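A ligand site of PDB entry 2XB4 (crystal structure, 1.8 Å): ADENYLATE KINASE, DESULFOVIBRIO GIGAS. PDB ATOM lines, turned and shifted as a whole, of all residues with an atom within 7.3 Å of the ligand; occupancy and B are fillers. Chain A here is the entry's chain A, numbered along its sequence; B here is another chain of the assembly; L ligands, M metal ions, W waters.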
ATOM      1  N   GLY A   7     -16.044  30.895   7.819  1.00  0.00           N
ATOM      2  CA  GLY A   7     -15.132  30.016   7.051  1.00  0.00           C
ATOM      3  C   GLY A   7     -15.701  28.585   7.071  1.00  0.00           C
ATOM      4  O   GLY A   7     -16.497  28.246   7.984  1.00  0.00           O
ATOM      5  N   PRO A   8     -15.308  27.763   6.087  1.00  0.00           N
ATOM      6  CA  PRO A   8     -15.854  26.401   5.951  1.00  0.00           C
ATOM      7  C   PRO A   8     -15.134  25.496   6.958  1.00  0.00           C
ATOM      8  O   PRO A   8     -14.037  25.866   7.448  1.00  0.00           O
ATOM      9  CB  PRO A   8     -15.376  25.957   4.570  1.00  0.00           C
ATOM     10  CG  PRO A   8     -14.132  26.764   4.279  1.00  0.00           C
ATOM     11  CD  PRO A   8     -14.406  28.140   4.968  1.00  0.00           C
ATOM     12  N   ASN A   9     -15.695  24.326   7.203  1.00  0.00           N
ATOM     13  CA  ASN A   9     -14.907  23.287   7.877  1.00  0.00           C
ATOM     14  C   ASN A   9     -13.628  22.997   7.090  1.00  0.00           C
ATOM     15  O   ASN A   9     -13.678  22.958   5.851  1.00  0.00           O
ATOM     16  CB  ASN A   9     -15.756  22.011   8.010  1.00  0.00           C
ATOM     17  CG  ASN A   9     -16.876  22.149   9.120  1.00  0.00           C
ATOM     18  OD1 ASN A   9     -16.884  23.074   9.980  1.00  0.00           O
ATOM     19  ND2 ASN A   9     -17.749  21.234   9.120  1.00  0.00           N
ATOM     20  N   GLY A  10     -12.480  22.835   7.757  1.00  0.00           N
ATOM     21  CA  GLY A  10     -11.226  22.585   7.021  1.00  0.00           C
ATOM     22  C   GLY A  10     -10.369  23.868   6.879  1.00  0.00           C
ATOM     23  O   GLY A  10      -9.230  23.817   6.365  1.00  0.00           O
ATOM     24  N   SER A  11     -10.858  25.010   7.332  1.00  0.00           N
ATOM     25  CA  SER A  11     -10.154  26.321   7.129  1.00  0.00           C
ATOM     26  C   SER A  11      -9.399  26.829   8.380  1.00  0.00           C
ATOM     27  O   SER A  11      -8.820  27.921   8.344  1.00  0.00           O
ATOM     28  CB  SER A  11     -11.109  27.462   6.694  1.00  0.00           C
ATOM     29  OG  SER A  11     -12.064  27.784   7.712  1.00  0.00           O
ATOM     30  N   GLY A  12      -9.431  26.085   9.499  1.00  0.00           N
ATOM     31  CA  GLY A  12      -8.685  26.551  10.721  1.00  0.00           C
ATOM     32  C   GLY A  12      -9.370  27.741  11.421  1.00  0.00           C
ATOM     33  O   GLY A  12      -8.746  28.467  12.175  1.00  0.00           O
ATOM     34  N   LYS A  13     -10.674  27.884  11.163  1.00  0.00           N
ATOM     35  CA  LYS A  13     -11.468  29.037  11.592  1.00  0.00           C
ATOM     36  C   LYS A  13     -11.463  29.230  13.177  1.00  0.00           C
ATOM     37  O   LYS A  13     -11.424  30.373  13.666  1.00  0.00           O
ATOM     38  CB  LYS A  13     -12.924  28.863  11.110  1.00  0.00           C
ATOM     39  CG  LYS A  13     -13.745  30.041  11.479  1.00  0.00           C
ATOM     40  CD  LYS A  13     -15.097  30.073  10.868  1.00  0.00           C
ATOM     41  CE  LYS A  13     -15.803  28.742  11.031  1.00  0.00           C
ATOM     42  NZ  LYS A  13     -16.626  28.696  12.230  1.00  0.00           N
ATOM     43  N   GLY A  14     -11.579  28.118  13.938  1.00  0.00           N
ATOM     44  CA  GLY A  14     -11.615  28.200  15.431  1.00  0.00           C
ATOM     45  C   GLY A  14     -10.287  28.696  15.975  1.00  0.00           C
ATOM     46  O   GLY A  14     -10.211  29.558  16.872  1.00  0.00           O
ATOM     47  N   THR A  15      -9.213  28.164  15.429  1.00  0.00           N
ATOM     48  CA  THR A  15      -7.889  28.578  15.794  1.00  0.00           C
ATOM     49  C   THR A  15      -7.667  30.062  15.613  1.00  0.00           C
ATOM     50  O   THR A  15      -7.139  30.735  16.503  1.00  0.00           O
ATOM     51  CB  THR A  15      -6.835  27.796  15.010  1.00  0.00           C
ATOM     52  OG1 THR A  15      -7.050  26.414  15.246  1.00  0.00           O
ATOM     53  CG2 THR A  15      -5.419  28.157  15.526  1.00  0.00           C
ATOM     54  N   GLN A  16      -8.049  30.576  14.447  1.00  0.00           N
ATOM     55  CA  GLN A  16      -7.898  32.010  14.129  1.00  0.00           C
ATOM     56  C   GLN A  16      -8.787  32.880  14.965  1.00  0.00           C
ATOM     57  O   GLN A  16      -8.335  33.923  15.461  1.00  0.00           O
ATOM     58  CB  GLN A  16      -8.133  32.335  12.624  1.00  0.00           C
ATOM     59  CG  GLN A  16      -7.130  31.689  11.669  1.00  0.00           C
ATOM     60  CD  GLN A  16      -5.673  32.031  12.053  1.00  0.00           C
ATOM     61  OE1 GLN A  16      -4.826  31.140  12.034  1.00  0.00           O
ATOM     62  NE2 GLN A  16      -5.380  33.309  12.425  1.00  0.00           N
ATOM     63  N   ASP A  83     -19.442  33.582  15.685  1.00  0.00           N
ATOM     64  CA  ASP A  83     -18.834  32.541  14.889  1.00  0.00           C
ATOM     65  C   ASP A  83     -19.953  31.499  14.676  1.00  0.00           C
ATOM     66  O   ASP A  83     -20.458  30.937  15.610  1.00  0.00           O
ATOM     67  CB  ASP A  83     -17.682  32.016  15.747  1.00  0.00           C
ATOM     68  CG  ASP A  83     -16.978  30.852  15.173  1.00  0.00           C
ATOM     69  OD1 ASP A  83     -17.405  30.353  14.125  1.00  0.00           O
ATOM     70  OD2 ASP A  83     -15.944  30.420  15.766  1.00  0.00           O
ATOM     71  N   ILE A 112     -12.418  33.545   5.945  1.00  0.00           N
ATOM     72  CA  ILE A 112     -11.278  32.706   5.569  1.00  0.00           C
ATOM     73  C   ILE A 112     -11.648  31.977   4.247  1.00  0.00           C
ATOM     74  O   ILE A 112     -12.647  31.268   4.196  1.00  0.00           O
ATOM     75  CB  ILE A 112     -10.948  31.692   6.657  1.00  0.00           C
ATOM     76  CG1 ILE A 112     -10.726  32.452   7.992  1.00  0.00           C
ATOM     77  CG2 ILE A 112      -9.659  30.877   6.191  1.00  0.00           C
ATOM     78  CD1 ILE A 112     -10.629  31.525   9.169  1.00  0.00           C
ATOM     79  N   LEU A 114     -10.962  29.437   1.092  1.00  0.00           N
ATOM     80  CA  LEU A 114     -10.258  28.207   0.731  1.00  0.00           C
ATOM     81  C   LEU A 114     -11.119  27.531  -0.375  1.00  0.00           C
ATOM     82  O   LEU A 114     -12.336  27.481  -0.222  1.00  0.00           O
ATOM     83  CB  LEU A 114     -10.214  27.333   2.035  1.00  0.00           C
ATOM     84  CG  LEU A 114      -9.210  26.228   2.199  1.00  0.00           C
ATOM     85  CD1 LEU A 114      -7.881  26.989   2.346  1.00  0.00           C
ATOM     86  CD2 LEU A 114      -9.443  25.508   3.442  1.00  0.00           C
ATOM     87  N   ALA A 119     -10.414  22.458   1.205  1.00  0.00           N
ATOM     88  CA  ALA A 119     -11.035  22.283   2.518  1.00  0.00           C
ATOM     89  C   ALA A 119     -11.336  20.773   2.807  1.00  0.00           C
ATOM     90  O   ALA A 119     -11.047  20.258   3.898  1.00  0.00           O
ATOM     91  CB  ALA A 119     -12.288  23.179   2.571  1.00  0.00           C
ATOM     92  N   ARG A 122      -8.076  18.812   3.293  1.00  0.00           N
ATOM     93  CA  ARG A 122      -7.511  19.090   4.644  1.00  0.00           C
ATOM     94  C   ARG A 122      -8.220  18.362   5.792  1.00  0.00           C
ATOM     95  O   ARG A 122      -7.545  18.023   6.764  1.00  0.00           O
ATOM     96  CB  ARG A 122      -7.501  20.564   4.949  1.00  0.00           C
ATOM     97  CG  ARG A 122      -6.480  21.264   4.137  1.00  0.00           C
ATOM     98  CD  ARG A 122      -6.422  22.740   4.454  1.00  0.00           C
ATOM     99  NE  ARG A 122      -5.279  23.228   3.651  1.00  0.00           N
ATOM    100  CZ  ARG A 122      -4.419  24.160   4.019  1.00  0.00           C
ATOM    101  NH1 ARG A 122      -4.536  24.731   5.207  1.00  0.00           N
ATOM    102  NH2 ARG A 122      -3.400  24.505   3.190  1.00  0.00           N
ATOM    103  N   ILE A 123      -9.556  18.203   5.741  1.00  0.00           N
ATOM    104  CA  ILE A 123     -10.221  17.475   6.786  1.00  0.00           C
ATOM    105  C   ILE A 123      -9.809  15.979   6.679  1.00  0.00           C
ATOM    106  O   ILE A 123      -9.481  15.343   7.688  1.00  0.00           O
ATOM    107  CB  ILE A 123     -11.744  17.595   6.641  1.00  0.00           C
ATOM    108  CG1 ILE A 123     -12.187  19.070   6.836  1.00  0.00           C
ATOM    109  CG2 ILE A 123     -12.511  16.616   7.583  1.00  0.00           C
ATOM    110  CD1 ILE A 123     -13.586  19.388   6.155  1.00  0.00           C
ATOM    111  N   ARG A 126      -6.192  14.630   7.885  1.00  0.00           N
ATOM    112  CA  ARG A 126      -5.716  14.635   9.282  1.00  0.00           C
ATOM    113  C   ARG A 126      -5.360  13.230   9.773  1.00  0.00           C
ATOM    114  O   ARG A 126      -6.143  12.268   9.541  1.00  0.00           O
ATOM    115  CB  ARG A 126      -6.832  15.143  10.192  1.00  0.00           C
ATOM    116  CG  ARG A 126      -7.322  16.662   9.947  1.00  0.00           C
ATOM    117  CD  ARG A 126      -8.678  16.928  10.635  1.00  0.00           C
ATOM    118  NE  ARG A 126      -9.010  18.348  10.511  1.00  0.00           N
ATOM    119  CZ  ARG A 126     -10.232  18.868  10.680  1.00  0.00           C
ATOM    120  NH1 ARG A 126     -11.240  18.049  11.010  1.00  0.00           N
ATOM    121  NH2 ARG A 126     -10.446  20.194  10.532  1.00  0.00           N
ATOM    122  N   CYS B 129     -11.156  17.588  20.347  1.00  0.00           N
ATOM    123  CA  CYS B 129     -12.145  18.389  19.667  1.00  0.00           C
ATOM    124  C   CYS B 129     -12.575  17.792  18.318  1.00  0.00           C
ATOM    125  O   CYS B 129     -11.737  17.467  17.457  1.00  0.00           O
ATOM    126  CB  CYS B 129     -11.553  19.806  19.458  1.00  0.00           C
ATOM    127  SG  CYS B 129     -12.637  20.969  18.503  1.00  0.00           S
ATOM    128  N   LYS B 130     -13.882  17.698  18.123  1.00  0.00           N
ATOM    129  CA  LYS B 130     -14.464  17.215  16.870  1.00  0.00           C
ATOM    130  C   LYS B 130     -14.083  18.071  15.681  1.00  0.00           C
ATOM    131  O   LYS B 130     -13.875  17.552  14.572  1.00  0.00           O
ATOM    132  CB  LYS B 130     -15.991  17.130  16.992  1.00  0.00           C
ATOM    133  CG  LYS B 130     -16.578  16.073  16.031  1.00  0.00           C
ATOM    134  CD  LYS B 130     -18.127  15.793  16.167  1.00  0.00           C
ATOM    135  CE  LYS B 130     -19.013  16.976  15.651  1.00  0.00           C
ATOM    136  NZ  LYS B 130     -19.931  16.619  14.460  1.00  0.00           N
ATOM    137  N   ASN B 131     -13.968  19.390  15.902  1.00  0.00           N
ATOM    138  CA  ASN B 131     -13.749  20.309  14.761  1.00  0.00           C
ATOM    139  C   ASN B 131     -12.287  20.316  14.341  1.00  0.00           C
ATOM    140  O   ASN B 131     -11.975  20.470  13.141  1.00  0.00           O
ATOM    141  CB  ASN B 131     -14.132  21.768  15.096  1.00  0.00           C
ATOM    142  CG  ASN B 131     -15.632  21.960  15.374  1.00  0.00           C
ATOM    143  OD1 ASN B 131     -16.470  21.191  14.914  1.00  0.00           O
ATOM    144  ND2 ASN B 131     -15.960  23.015  16.092  1.00  0.00           N
ATOM    145  N   ASN B 132     -11.390  20.248  15.331  1.00  0.00           N
ATOM    146  CA  ASN B 132      -9.959  20.259  14.975  1.00  0.00           C
ATOM    147  C   ASN B 132      -9.158  19.525  16.047  1.00  0.00           C
ATOM    148  O   ASN B 132      -9.073  20.004  17.190  1.00  0.00           O
ATOM    149  CB  ASN B 132      -9.481  21.725  14.878  1.00  0.00           C
ATOM    150  CG  ASN B 132      -8.014  21.848  14.344  1.00  0.00           C
ATOM    151  OD1 ASN B 132      -7.192  20.969  14.557  1.00  0.00           O
ATOM    152  ND2 ASN B 132      -7.710  22.974  13.711  1.00  0.00           N
ATOM    153  N   PRO B 133      -8.574  18.367  15.701  1.00  0.00           N
ATOM    154  CA  PRO B 133      -7.953  17.529  16.770  1.00  0.00           C
ATOM    155  C   PRO B 133      -6.664  18.174  17.342  1.00  0.00           C
ATOM    156  O   PRO B 133      -6.198  17.747  18.365  1.00  0.00           O
ATOM    157  CB  PRO B 133      -7.637  16.214  16.012  1.00  0.00           C
ATOM    158  CG  PRO B 133      -7.351  16.667  14.539  1.00  0.00           C
ATOM    159  CD  PRO B 133      -8.415  17.804  14.357  1.00  0.00           C
ATOM    160  N   ASN B 134      -6.177  19.242  16.727  1.00  0.00           N
ATOM    161  CA  ASN B 134      -4.951  19.966  17.194  1.00  0.00           C
ATOM    162  C   ASN B 134      -5.285  20.734  18.475  1.00  0.00           C
ATOM    163  O   ASN B 134      -4.331  21.039  19.226  1.00  0.00           O
ATOM    164  CB  ASN B 134      -4.415  21.052  16.217  1.00  0.00           C
ATOM    165  CG  ASN B 134      -3.931  20.492  14.828  1.00  0.00           C
ATOM    166  OD1 ASN B 134      -3.673  19.283  14.666  1.00  0.00           O
ATOM    167  ND2 ASN B 134      -3.733  21.414  13.846  1.00  0.00           N
ATOM    168  N   HIS B 135      -6.560  21.076  18.721  1.00  0.00           N
ATOM    169  CA  HIS B 135      -6.944  22.027  19.859  1.00  0.00           C
ATOM    170  C   HIS B 135      -6.741  21.365  21.244  1.00  0.00           C
ATOM    171  O   HIS B 135      -7.496  20.488  21.568  1.00  0.00           O
ATOM    172  CB  HIS B 135      -8.441  22.458  19.753  1.00  0.00           C
ATOM    173  CG  HIS B 135      -8.737  23.332  18.553  1.00  0.00           C
ATOM    174  ND1 HIS B 135     -10.027  23.647  18.168  1.00  0.00           N
ATOM    175  CD2 HIS B 135      -7.914  24.016  17.716  1.00  0.00           C
ATOM    176  CE1 HIS B 135      -9.985  24.419  17.080  1.00  0.00           C
ATOM    177  NE2 HIS B 135      -8.717  24.677  16.806  1.00  0.00           N
ATOM    178  N   CYS B 154     -12.460  26.544  20.367  1.00  0.00           N
ATOM    179  CA  CYS B 154     -13.465  26.865  19.337  1.00  0.00           C
ATOM    180  C   CYS B 154     -14.901  26.523  19.702  1.00  0.00           C
ATOM    181  O   CYS B 154     -15.821  26.839  18.921  1.00  0.00           O
ATOM    182  CB  CYS B 154     -13.125  26.197  17.985  1.00  0.00           C
ATOM    183  SG  CYS B 154     -13.469  24.352  18.069  1.00  0.00           S
ATOM    184  N   GLY B 156     -16.160  23.547  19.941  1.00  0.00           N
ATOM    185  CA  GLY B 156     -16.588  22.259  19.361  1.00  0.00           C
ATOM    186  C   GLY B 156     -16.821  21.184  20.421  1.00  0.00           C
ATOM    187  O   GLY B 156     -16.331  21.249  21.547  1.00  0.00           O
HETATM  188  O1  LIG L   1     -10.262  23.041  10.137  1.00  0.00           O
HETATM  189  O2  LIG L   1     -10.089  24.015  12.173  1.00  0.00           O
HETATM  190  C1  LIG L   1     -10.721  23.534  11.208  1.00  0.00           C
HETATM  191  C2  LIG L   1     -12.168  23.711  11.035  1.00  0.00           C
HETATM  192  O3  LIG L   1     -12.980  22.607  10.685  1.00  0.00           O
HETATM  193  C3  LIG L   1     -12.769  24.995  11.489  1.00  0.00           C
HETATM  194  O4  LIG L   1     -12.509  25.529  10.167  1.00  0.00           O
HETATM  195  C4  LIG L   1     -14.221  24.925  11.690  1.00  0.00           C
HETATM  196  O5  LIG L   1     -14.614  24.600  12.825  1.00  0.00           O
HETATM  197  O6  LIG L   1     -14.950  25.203  10.742  1.00  0.00           O
HETATM  198 ZN    ZN M   1     -11.765  23.053  19.021  1.00  0.00          ZN
HETATM  199  O   HOH W   1     -14.981  27.139  14.962  1.00  0.00           O
HETATM  200  O   HOH W   2     -17.776  26.136  11.349  1.00  0.00           O
HETATM  201  O   HOH W   3      -7.751  22.761   9.421  1.00  0.00           O
HETATM  202  O   HOH W   4     -12.374  24.965  14.855  1.00  0.00           O
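The guanidinium group of Arg 126 lies within hydrogen-bond range of the backbone carbonyl oxygen of Asn 131 of chain B, 3.0 Å away. SG of Cys 129 of chain B sits close to N of Asn 132 of chain B (3.5 Å). The backbone NH (N) of Asn 134 of chain B is in hydrogen-bond range of the side-chain amide oxygen (OD1) of Asn 132 of chain B. The side-chain hydroxyl (OG) of Ser 11 lies within hydrogen-bond range of the backbone carbonyl oxygen (O) of Pro 8 (2.8 Å). NZ of Lys 13 is in salt-bridge range of OD1 of Asp 83 (2.6 Å). The side-chain sulfur of Cys 154 of chain B lies close to the side-chain amide nitrogen of Asn 131 of chain B. The backbone NH of Asn 131 of chain B sits close to the side-chain sulfur of Cys 129 of chain B, at 3.3 Å.
NH2 of Arg 126 lies within salt-bridge range of O1 of the ligand (2.9 Å). The side-chain amide oxygen (OD1) of Asn 9 lies close to an oxygen (O6) of the ligand. The backbone NH (N) of Gly 10 is in hydrogen-bond range of an oxygen (O3) of the ligand (3.0 Å). An oxygen (O2) of the ligand is in hydrogen-bond range of the side-chain amide nitrogen (ND2) of Asn 132 of chain B (3.0 Å). O4 of the ligand sits at hydrogen-bond distance from O of Pro 8 (3.1 Å). The backbone NH (N) of Lys 13 lies within hydrogen-bond range of an oxygen (O4) of the ligand, 3.1 Å away. The backbone NH of Gly 12 sits at hydrogen-bond distance from an oxygen (O4) of the ligand (3.2 Å). The backbone NH of Ser 11 sits at hydrogen-bond distance from an oxygen (O4) of the ligand (3.3 Å). The side-chain hydroxyl (OG) of Ser 11 is in hydrogen-bond range of an oxygen (O4) of the ligand, at 3.4 Å. O3 of the ligand is in hydrogen-bond range of O of Asn 131 of chain B, 3.4 Å away.
Water W2 lies within hydrogen-bond range of NZ of Lys 13 (2.9 Å), O6 of the ligand (3.0 Å) and OD1 of Asn 9 (3.5 Å). Water W4 lies within hydrogen-bond range of an oxygen (O5) of the ligand (3.0 Å) and the backbone NH (N) of Gly 14 (3.4 Å).
Within 4 Å of the ligand: Pro 8, Asn 9, Gly 10, Ser 11, Gly 12, Lys 13, Arg 126, Asn 131 of chain B and Asn 132 of chain B. The nearest printed residue that does not touch the ligand is Gly 14 (4.1 Å).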
